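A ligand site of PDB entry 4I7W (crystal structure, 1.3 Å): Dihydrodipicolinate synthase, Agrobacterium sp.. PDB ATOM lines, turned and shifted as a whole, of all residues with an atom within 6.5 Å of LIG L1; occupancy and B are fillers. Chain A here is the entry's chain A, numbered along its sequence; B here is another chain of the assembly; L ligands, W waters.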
ATOM      1  N   VAL A  56     -20.095   3.895  18.733  1.00  0.00           N
ATOM      2  CA  VAL A  56     -21.197   4.140  17.794  1.00  0.00           C
ATOM      3  C   VAL A  56     -22.518   4.529  18.478  1.00  0.00           C
ATOM      4  O   VAL A  56     -23.587   3.975  18.177  1.00  0.00           O
ATOM      5  CB  VAL A  56     -21.393   2.983  16.769  1.00  0.00           C
ATOM      6  CG1 VAL A  56     -22.138   3.477  15.549  1.00  0.00           C
ATOM      7  CG2 VAL A  56     -20.064   2.408  16.330  1.00  0.00           C
ATOM      8  N   GLU A  61     -21.260   9.155  15.560  1.00  0.00           N
ATOM      9  CA  GLU A  61     -21.834   9.391  14.222  1.00  0.00           C
ATOM     10  C   GLU A  61     -22.529   8.155  13.645  1.00  0.00           C
ATOM     11  O   GLU A  61     -22.459   7.887  12.445  1.00  0.00           O
ATOM     12  CB  GLU A  61     -20.800   9.996  13.269  1.00  0.00           C
ATOM     13  CG  GLU A  61     -20.425  11.427  13.639  1.00  0.00           C
ATOM     14  CD  GLU A  61     -19.284  11.974  12.813  1.00  0.00           C
ATOM     15  OE1 GLU A  61     -19.524  12.390  11.659  1.00  0.00           O
ATOM     16  OE2 GLU A  61     -18.146  12.010  13.319  1.00  0.00           O
ATOM     17  N   SER A  62     -23.210   7.431  14.524  1.00  0.00           N
ATOM     18  CA  SER A  62     -24.052   6.306  14.118  1.00  0.00           C
ATOM     19  C   SER A  62     -24.921   6.593  12.876  1.00  0.00           C
ATOM     20  O   SER A  62     -25.025   5.731  12.005  1.00  0.00           O
ATOM     21  CB  SER A  62     -24.927   5.829  15.294  1.00  0.00           C
ATOM     22  OG  SER A  62     -25.767   4.754  14.896  1.00  0.00           O
ATOM     23  N   PRO A  63     -25.550   7.795  12.787  1.00  0.00           N
ATOM     24  CA  PRO A  63     -26.420   8.032  11.631  1.00  0.00           C
ATOM     25  C   PRO A  63     -25.742   8.005  10.256  1.00  0.00           C
ATOM     26  O   PRO A  63     -26.404   7.703   9.264  1.00  0.00           O
ATOM     27  CB  PRO A  63     -26.985   9.425  11.896  1.00  0.00           C
ATOM     28  CG  PRO A  63     -26.911   9.588  13.367  1.00  0.00           C
ATOM     29  CD  PRO A  63     -25.635   8.905  13.750  1.00  0.00           C
ATOM     30  N   THR A  64     -24.452   8.312  10.197  1.00  0.00           N
ATOM     31  CA  THR A  64     -23.774   8.437   8.898  1.00  0.00           C
ATOM     32  C   THR A  64     -22.831   7.278   8.587  1.00  0.00           C
ATOM     33  O   THR A  64     -22.159   7.274   7.554  1.00  0.00           O
ATOM     34  CB  THR A  64     -23.049   9.778   8.750  1.00  0.00           C
ATOM     35  OG1 THR A  64     -22.144   9.951   9.843  1.00  0.00           O
ATOM     36  CG2 THR A  64     -24.053  10.926   8.716  1.00  0.00           C
ATOM     37  N   LEU A  65     -22.784   6.290   9.480  1.00  0.00           N
ATOM     38  CA  LEU A  65     -22.093   5.037   9.175  1.00  0.00           C
ATOM     39  C   LEU A  65     -23.049   4.085   8.480  1.00  0.00           C
ATOM     40  O   LEU A  65     -24.247   4.089   8.755  1.00  0.00           O
ATOM     41  CB  LEU A  65     -21.543   4.378  10.450  1.00  0.00           C
ATOM     42  CG  LEU A  65     -20.575   5.184  11.324  1.00  0.00           C
ATOM     43  CD1 LEU A  65     -20.127   4.355  12.511  1.00  0.00           C
ATOM     44  CD2 LEU A  65     -19.367   5.687  10.532  1.00  0.00           C
ATOM     45  N   SER A  66     -22.517   3.284   7.550  1.00  0.00           N
ATOM     46  CA  SER A  66     -23.265   2.154   7.002  1.00  0.00           C
ATOM     47  C   SER A  66     -23.397   1.109   8.101  1.00  0.00           C
ATOM     48  O   SER A  66     -22.722   1.190   9.128  1.00  0.00           O
ATOM     49  CB  SER A  66     -22.541   1.566   5.791  1.00  0.00           C
ATOM     50  OG  SER A  66     -21.350   0.910   6.195  1.00  0.00           O
ATOM     51  N   HIS A  67     -24.271   0.119   7.883  1.00  0.00           N
ATOM     52  CA  HIS A  67     -24.404  -0.972   8.832  1.00  0.00           C
ATOM     53  C   HIS A  67     -23.094  -1.750   8.984  1.00  0.00           C
ATOM     54  O   HIS A  67     -22.722  -2.134  10.087  1.00  0.00           O
ATOM     55  CB  HIS A  67     -25.570  -1.892   8.449  1.00  0.00           C
ATOM     56  CG  HIS A  67     -26.910  -1.233   8.590  1.00  0.00           C
ATOM     57  ND1 HIS A  67     -27.531  -0.586   7.536  1.00  0.00           N
ATOM     58  CD2 HIS A  67     -27.744  -1.110   9.651  1.00  0.00           C
ATOM     59  CE1 HIS A  67     -28.685  -0.097   7.947  1.00  0.00           C
ATOM     60  NE2 HIS A  67     -28.837  -0.404   9.220  1.00  0.00           N
ATOM     61  N   HIS A  70     -20.730   0.515  11.080  1.00  0.00           N
ATOM     62  CA  HIS A  70     -21.236   0.485  12.445  1.00  0.00           C
ATOM     63  C   HIS A  70     -20.749  -0.786  13.144  1.00  0.00           C
ATOM     64  O   HIS A  70     -20.150  -0.718  14.227  1.00  0.00           O
ATOM     65  CB  HIS A  70     -22.771   0.522  12.411  1.00  0.00           C
ATOM     66  CG  HIS A  70     -23.412   0.653  13.759  1.00  0.00           C
ATOM     67  ND1 HIS A  70     -24.466   1.499  13.996  1.00  0.00           N
ATOM     68  CD2 HIS A  70     -23.178   0.013  14.934  1.00  0.00           C
ATOM     69  CE1 HIS A  70     -24.845   1.398  15.257  1.00  0.00           C
ATOM     70  NE2 HIS A  70     -24.075   0.504  15.852  1.00  0.00           N
ATOM     71  N   GLY A  92     -28.729   1.380  18.422  1.00  0.00           N
ATOM     72  CA  GLY A  92     -29.953   2.145  18.249  1.00  0.00           C
ATOM     73  C   GLY A  92     -30.392   2.287  16.810  1.00  0.00           C
ATOM     74  O   GLY A  92     -29.573   2.421  15.902  1.00  0.00           O
ATOM     75  N   SER A  93     -31.705   2.242  16.611  1.00  0.00           N
ATOM     76  CA  SER A  93     -32.331   2.533  15.327  1.00  0.00           C
ATOM     77  C   SER A  93     -33.784   2.939  15.537  1.00  0.00           C
ATOM     78  O   SER A  93     -34.399   2.561  16.547  1.00  0.00           O
ATOM     79  CB  SER A  93     -32.275   1.325  14.388  1.00  0.00           C
ATOM     80  OG  SER A  93     -32.916   1.615  13.160  1.00  0.00           O
ATOM     81  N   ASN A  94     -34.333   3.687  14.589  1.00  0.00           N
ATOM     82  CA  ASN A  94     -35.767   3.978  14.587  1.00  0.00           C
ATOM     83  C   ASN A  94     -36.579   2.859  13.950  1.00  0.00           C
ATOM     84  O   ASN A  94     -37.808   2.926  13.876  1.00  0.00           O
ATOM     85  CB  ASN A  94     -36.042   5.325  13.915  1.00  0.00           C
ATOM     86  CG  ASN A  94     -35.588   5.371  12.466  1.00  0.00           C
ATOM     87  OD1 ASN A  94     -34.913   4.474  11.977  1.00  0.00           O
ATOM     88  ND2 ASN A  94     -35.965   6.436  11.768  1.00  0.00           N
ATOM     89  N   ASN A  95     -35.875   1.832  13.490  1.00  0.00           N
ATOM     90  CA  ASN A  95     -36.458   0.652  12.867  1.00  0.00           C
ATOM     91  C   ASN A  95     -36.108  -0.552  13.734  1.00  0.00           C
ATOM     92  O   ASN A  95     -34.928  -0.863  13.912  1.00  0.00           O
ATOM     93  CB  ASN A  95     -35.898   0.506  11.436  1.00  0.00           C
ATOM     94  CG  ASN A  95     -36.352  -0.763  10.740  1.00  0.00           C
ATOM     95  OD1 ASN A  95     -37.191  -1.522  11.234  1.00  0.00           O
ATOM     96  ND2 ASN A  95     -35.787  -1.010   9.560  1.00  0.00           N
ATOM     97  N   GLU A  98     -33.667  -3.128  12.353  1.00  0.00           N
ATOM     98  CA  GLU A  98     -32.267  -2.685  12.335  1.00  0.00           C
ATOM     99  C   GLU A  98     -31.634  -2.741  13.718  1.00  0.00           C
ATOM    100  O   GLU A  98     -30.462  -3.112  13.854  1.00  0.00           O
ATOM    101  CB  GLU A  98     -32.143  -1.277  11.761  1.00  0.00           C
ATOM    102  CG  GLU A  98     -32.322  -1.175  10.260  1.00  0.00           C
ATOM    103  CD  GLU A  98     -32.256   0.270   9.788  1.00  0.00           C
ATOM    104  OE1 GLU A  98     -33.309   0.819   9.422  1.00  0.00           O
ATOM    105  OE2 GLU A  98     -31.151   0.847   9.810  1.00  0.00           O
ATOM    106  N   LEU A 102     -28.335  -4.946  14.638  1.00  0.00           N
ATOM    107  CA  LEU A 102     -27.154  -4.366  15.267  1.00  0.00           C
ATOM    108  C   LEU A 102     -26.866  -4.981  16.640  1.00  0.00           C
ATOM    109  O   LEU A 102     -25.706  -5.231  16.984  1.00  0.00           O
ATOM    110  CB  LEU A 102     -27.284  -2.848  15.371  1.00  0.00           C
ATOM    111  CG  LEU A 102     -27.307  -2.075  14.054  1.00  0.00           C
ATOM    112  CD1 LEU A 102     -27.795  -0.650  14.301  1.00  0.00           C
ATOM    113  CD2 LEU A 102     -25.945  -2.060  13.372  1.00  0.00           C
ATOM    114  N   TYR A 120     -36.432   7.579  16.601  1.00  0.00           N
ATOM    115  CA  TYR A 120     -36.466   8.966  16.167  1.00  0.00           C
ATOM    116  C   TYR A 120     -37.190   9.084  14.828  1.00  0.00           C
ATOM    117  O   TYR A 120     -37.296   8.112  14.080  1.00  0.00           O
ATOM    118  CB  TYR A 120     -35.027   9.499  16.035  1.00  0.00           C
ATOM    119  CG  TYR A 120     -34.089   8.488  15.410  1.00  0.00           C
ATOM    120  CD1 TYR A 120     -33.921   8.427  14.022  1.00  0.00           C
ATOM    121  CD2 TYR A 120     -33.411   7.558  16.197  1.00  0.00           C
ATOM    122  CE1 TYR A 120     -33.091   7.482  13.440  1.00  0.00           C
ATOM    123  CE2 TYR A 120     -32.572   6.604  15.620  1.00  0.00           C
ATOM    124  CZ  TYR A 120     -32.422   6.574  14.249  1.00  0.00           C
ATOM    125  OH  TYR A 120     -31.601   5.620  13.695  1.00  0.00           O
ATOM    126  N   SER B  93     -33.045  11.287   3.870  1.00  0.00           N
ATOM    127  CA  SER B  93     -32.227  10.612   4.869  1.00  0.00           C
ATOM    128  C   SER B  93     -31.537  11.638   5.742  1.00  0.00           C
ATOM    129  O   SER B  93     -31.315  12.778   5.332  1.00  0.00           O
ATOM    130  CB  SER B  93     -31.172   9.720   4.207  1.00  0.00           C
ATOM    131  OG  SER B  93     -30.340   9.122   5.199  1.00  0.00           O
ATOM    132  N   ASN B  94     -31.158  11.223   6.954  1.00  0.00           N
ATOM    133  CA  ASN B  94     -30.336  12.062   7.818  1.00  0.00           C
ATOM    134  C   ASN B  94     -28.843  11.923   7.502  1.00  0.00           C
ATOM    135  O   ASN B  94     -28.007  12.571   8.119  1.00  0.00           O
ATOM    136  CB  ASN B  94     -30.621  11.754   9.292  1.00  0.00           C
ATOM    137  CG  ASN B  94     -30.334  10.321   9.667  1.00  0.00           C
ATOM    138  OD1 ASN B  94     -30.093   9.462   8.822  1.00  0.00           O
ATOM    139  ND2 ASN B  94     -30.378  10.035  10.973  1.00  0.00           N
ATOM    140  N   ASN B  95     -28.538  11.057   6.532  1.00  0.00           N
ATOM    141  CA  ASN B  95     -27.188  10.820   6.049  1.00  0.00           C
ATOM    142  C   ASN B  95     -27.130  11.245   4.582  1.00  0.00           C
ATOM    143  O   ASN B  95     -27.846  10.681   3.740  1.00  0.00           O
ATOM    144  CB  ASN B  95     -26.841   9.342   6.224  1.00  0.00           C
ATOM    145  CG  ASN B  95     -25.501   8.952   5.610  1.00  0.00           C
ATOM    146  OD1 ASN B  95     -24.724   9.804   5.160  1.00  0.00           O
ATOM    147  ND2 ASN B  95     -25.230   7.654   5.593  1.00  0.00           N
ATOM    148  N   GLU B  98     -26.756   8.568   1.910  1.00  0.00           N
ATOM    149  CA  GLU B  98     -27.963   7.782   1.662  1.00  0.00           C
ATOM    150  C   GLU B  98     -28.984   8.551   0.830  1.00  0.00           C
ATOM    151  O   GLU B  98     -29.631   7.971  -0.046  1.00  0.00           O
ATOM    152  CB  GLU B  98     -28.605   7.333   2.973  1.00  0.00           C
ATOM    153  CG  GLU B  98     -27.870   6.247   3.708  1.00  0.00           C
ATOM    154  CD  GLU B  98     -28.522   5.913   5.035  1.00  0.00           C
ATOM    155  OE1 GLU B  98     -27.959   6.264   6.086  1.00  0.00           O
ATOM    156  OE2 GLU B  98     -29.623   5.320   5.020  1.00  0.00           O
ATOM    157  N   TYR B 120     -32.841  14.316  10.296  1.00  0.00           N
ATOM    158  CA  TYR B 120     -33.436  14.068  11.604  1.00  0.00           C
ATOM    159  C   TYR B 120     -32.412  13.406  12.526  1.00  0.00           C
ATOM    160  O   TYR B 120     -31.448  12.782  12.052  1.00  0.00           O
ATOM    161  CB  TYR B 120     -34.669  13.156  11.456  1.00  0.00           C
ATOM    162  CG  TYR B 120     -34.452  12.048  10.448  1.00  0.00           C
ATOM    163  CD1 TYR B 120     -33.907  10.821  10.833  1.00  0.00           C
ATOM    164  CD2 TYR B 120     -34.745  12.244   9.095  1.00  0.00           C
ATOM    165  CE1 TYR B 120     -33.682   9.813   9.911  1.00  0.00           C
ATOM    166  CE2 TYR B 120     -34.511  11.250   8.157  1.00  0.00           C
ATOM    167  CZ  TYR B 120     -33.974  10.045   8.564  1.00  0.00           C
ATOM    168  OH  TYR B 120     -33.750   9.060   7.623  1.00  0.00           O
ATOM    169  N   TYR B 121     -32.647  13.529  13.824  1.00  0.00           N
ATOM    170  CA  TYR B 121     -31.819  12.961  14.896  1.00  0.00           C
ATOM    171  C   TYR B 121     -30.464  13.651  15.130  1.00  0.00           C
ATOM    172  O   TYR B 121     -30.161  14.018  16.261  1.00  0.00           O
ATOM    173  CB  TYR B 121     -31.662  11.430  14.798  1.00  0.00           C
ATOM    174  CG  TYR B 121     -31.032  10.853  16.038  1.00  0.00           C
ATOM    175  CD1 TYR B 121     -31.788  10.610  17.184  1.00  0.00           C
ATOM    176  CD2 TYR B 121     -29.667  10.585  16.086  1.00  0.00           C
ATOM    177  CE1 TYR B 121     -31.212  10.100  18.340  1.00  0.00           C
ATOM    178  CE2 TYR B 121     -29.074  10.072  17.243  1.00  0.00           C
ATOM    179  CZ  TYR B 121     -29.863   9.837  18.363  1.00  0.00           C
ATOM    180  OH  TYR B 121     -29.285   9.335  19.507  1.00  0.00           O
HETATM  181  N1  LIG L   1     -28.904   6.933   8.638  1.00  0.00           N
HETATM  182  C1  LIG L   1     -29.768   5.855   9.207  1.00  0.00           C
HETATM  183  C2  LIG L   1     -30.223   6.193  10.621  1.00  0.00           C
HETATM  184  O1  LIG L   1     -29.774   7.176  11.218  1.00  0.00           O
HETATM  185  C3  LIG L   1     -29.049   4.496   9.163  1.00  0.00           C
HETATM  186  C4  LIG L   1     -27.815   4.354  10.065  1.00  0.00           C
HETATM  187  C5  LIG L   1     -27.355   2.887  10.137  1.00  0.00           C
HETATM  188  C6  LIG L   1     -26.079   2.695  10.944  1.00  0.00           C
HETATM  189  N2  LIG L   1     -26.155   3.214  12.337  1.00  0.00           N
HETATM  190  O2  LIG L   1     -31.062   5.486  11.184  1.00  0.00           O
HETATM  191  N1  LG2 L   2     -34.156   3.475   9.455  1.00  0.00           N
HETATM  192  C1  LG2 L   2     -33.203   4.349   8.722  1.00  0.00           C
HETATM  193  C2  LG2 L   2     -33.686   5.790   8.671  1.00  0.00           C
HETATM  194  O1  LG2 L   2     -32.944   6.682   8.251  1.00  0.00           O
HETATM  195  C3  LG2 L   2     -32.924   3.811   7.307  1.00  0.00           C
HETATM  196  C4  LG2 L   2     -34.102   3.849   6.328  1.00  0.00           C
HETATM  197  C5  LG2 L   2     -33.619   3.565   4.894  1.00  0.00           C
HETATM  198  C6  LG2 L   2     -34.763   3.491   3.896  1.00  0.00           C
HETATM  199  N2  LG2 L   2     -35.573   4.743   3.845  1.00  0.00           N
HETATM  200  O2  LG2 L   2     -34.821   6.084   9.057  1.00  0.00           O
HETATM  201  O   HOH W   1     -31.027   2.781  11.619  1.00  0.00           O
HETATM  202  O   HOH W   2     -28.875   3.005  13.333  1.00  0.00           O
HETATM  203  O   HOH W   3     -28.449   6.108  13.664  1.00  0.00           O
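O2 of LIG L1 sits at hydrogen-bond distance from OH of Tyr 120 of chain A (2.6 Å). A nitrogen (N1) of LIG L1 lies within hydrogen-bond range of the backbone carbonyl oxygen (O) of Pro 63, at 2.7 Å. A nitrogen (N2) of LIG L1 is in hydrogen-bond range of the backbone carbonyl oxygen (O) of Ser 62, 2.8 Å away. The side-chain hydroxyl of Ser 62 lies within hydrogen-bond range of a nitrogen (N2) of LIG L1. OD1 of Asn 94 of chain B sits at hydrogen-bond distance from N1 of LIG L1 (2.8 Å). OE1 of Glu 98 of chain B lies within salt-bridge range of N1 of LIG L1 (2.8 Å). A ring nitrogen (ND1) of His 70 lies within hydrogen-bond range of a nitrogen (N2) of LIG L1 (2.9 Å). OD1 of Asn 94 of chain A sits at hydrogen-bond distance from N1 of LG2 L2 (2.8 Å). N1 of LG2 L2 is in salt-bridge range of OE1 of Glu 98 of chain A (2.8 Å). O1 of LG2 L2 lies within hydrogen-bond range of OH of Tyr 120 of chain B (2.6 Å).
The backbone carbonyl oxygen (O) of Tyr 120 of chain A sits close to the side-chain amide nitrogen (ND2) of Asn 94 of chain A (3.2 Å). ND2 of Asn 94 of chain B sits close to O of Tyr 120 of chain B (3.1 Å). The side-chain amide nitrogen (ND2) of Asn 95 of chain B sits at hydrogen-bond distance from the side-chain carboxylate (OE1) of Glu 98 of chain B, at 3.1 Å. A ring nitrogen (NE2) of His 67 sits at hydrogen-bond distance from the side-chain carboxylate (OE2) of Glu 98 of chain A. The backbone NH (N) of Asn 95 of chain B is in hydrogen-bond range of the side-chain hydroxyl (OG) of Ser 93 of chain B, at 3.0 Å.
O of Leu 65 touches C6 of LIG L1, 3.2 Å away. His 67 touches LIG L1. Asn 95 of chain B touches LIG L1 (CB to N1, 3.99 Å). Within 4 Å of LIG L1: Ser 62, Pro 63, Leu 65, His 67, His 70, Tyr 120 of chain A, Asn 94 of chain B, Asn 95 of chain B and Glu 98 of chain B.
Water W1 lies within hydrogen-bond range of OE2 of Glu 98 of chain A (2.7 Å), OG of Ser 93 of chain A (2.7 Å) and O2 of LIG L1 (2.7 Å). Water W2 bridges O of Gly 92 (2.7 Å) and N2 of LIG L1 (2.9 Å). Water W3 lies within hydrogen-bond range of O1 of LIG L1 (3.0 Å), OH of Tyr 120 of chain A (3.2 Å) and OG of Ser 62 (3.2 Å).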
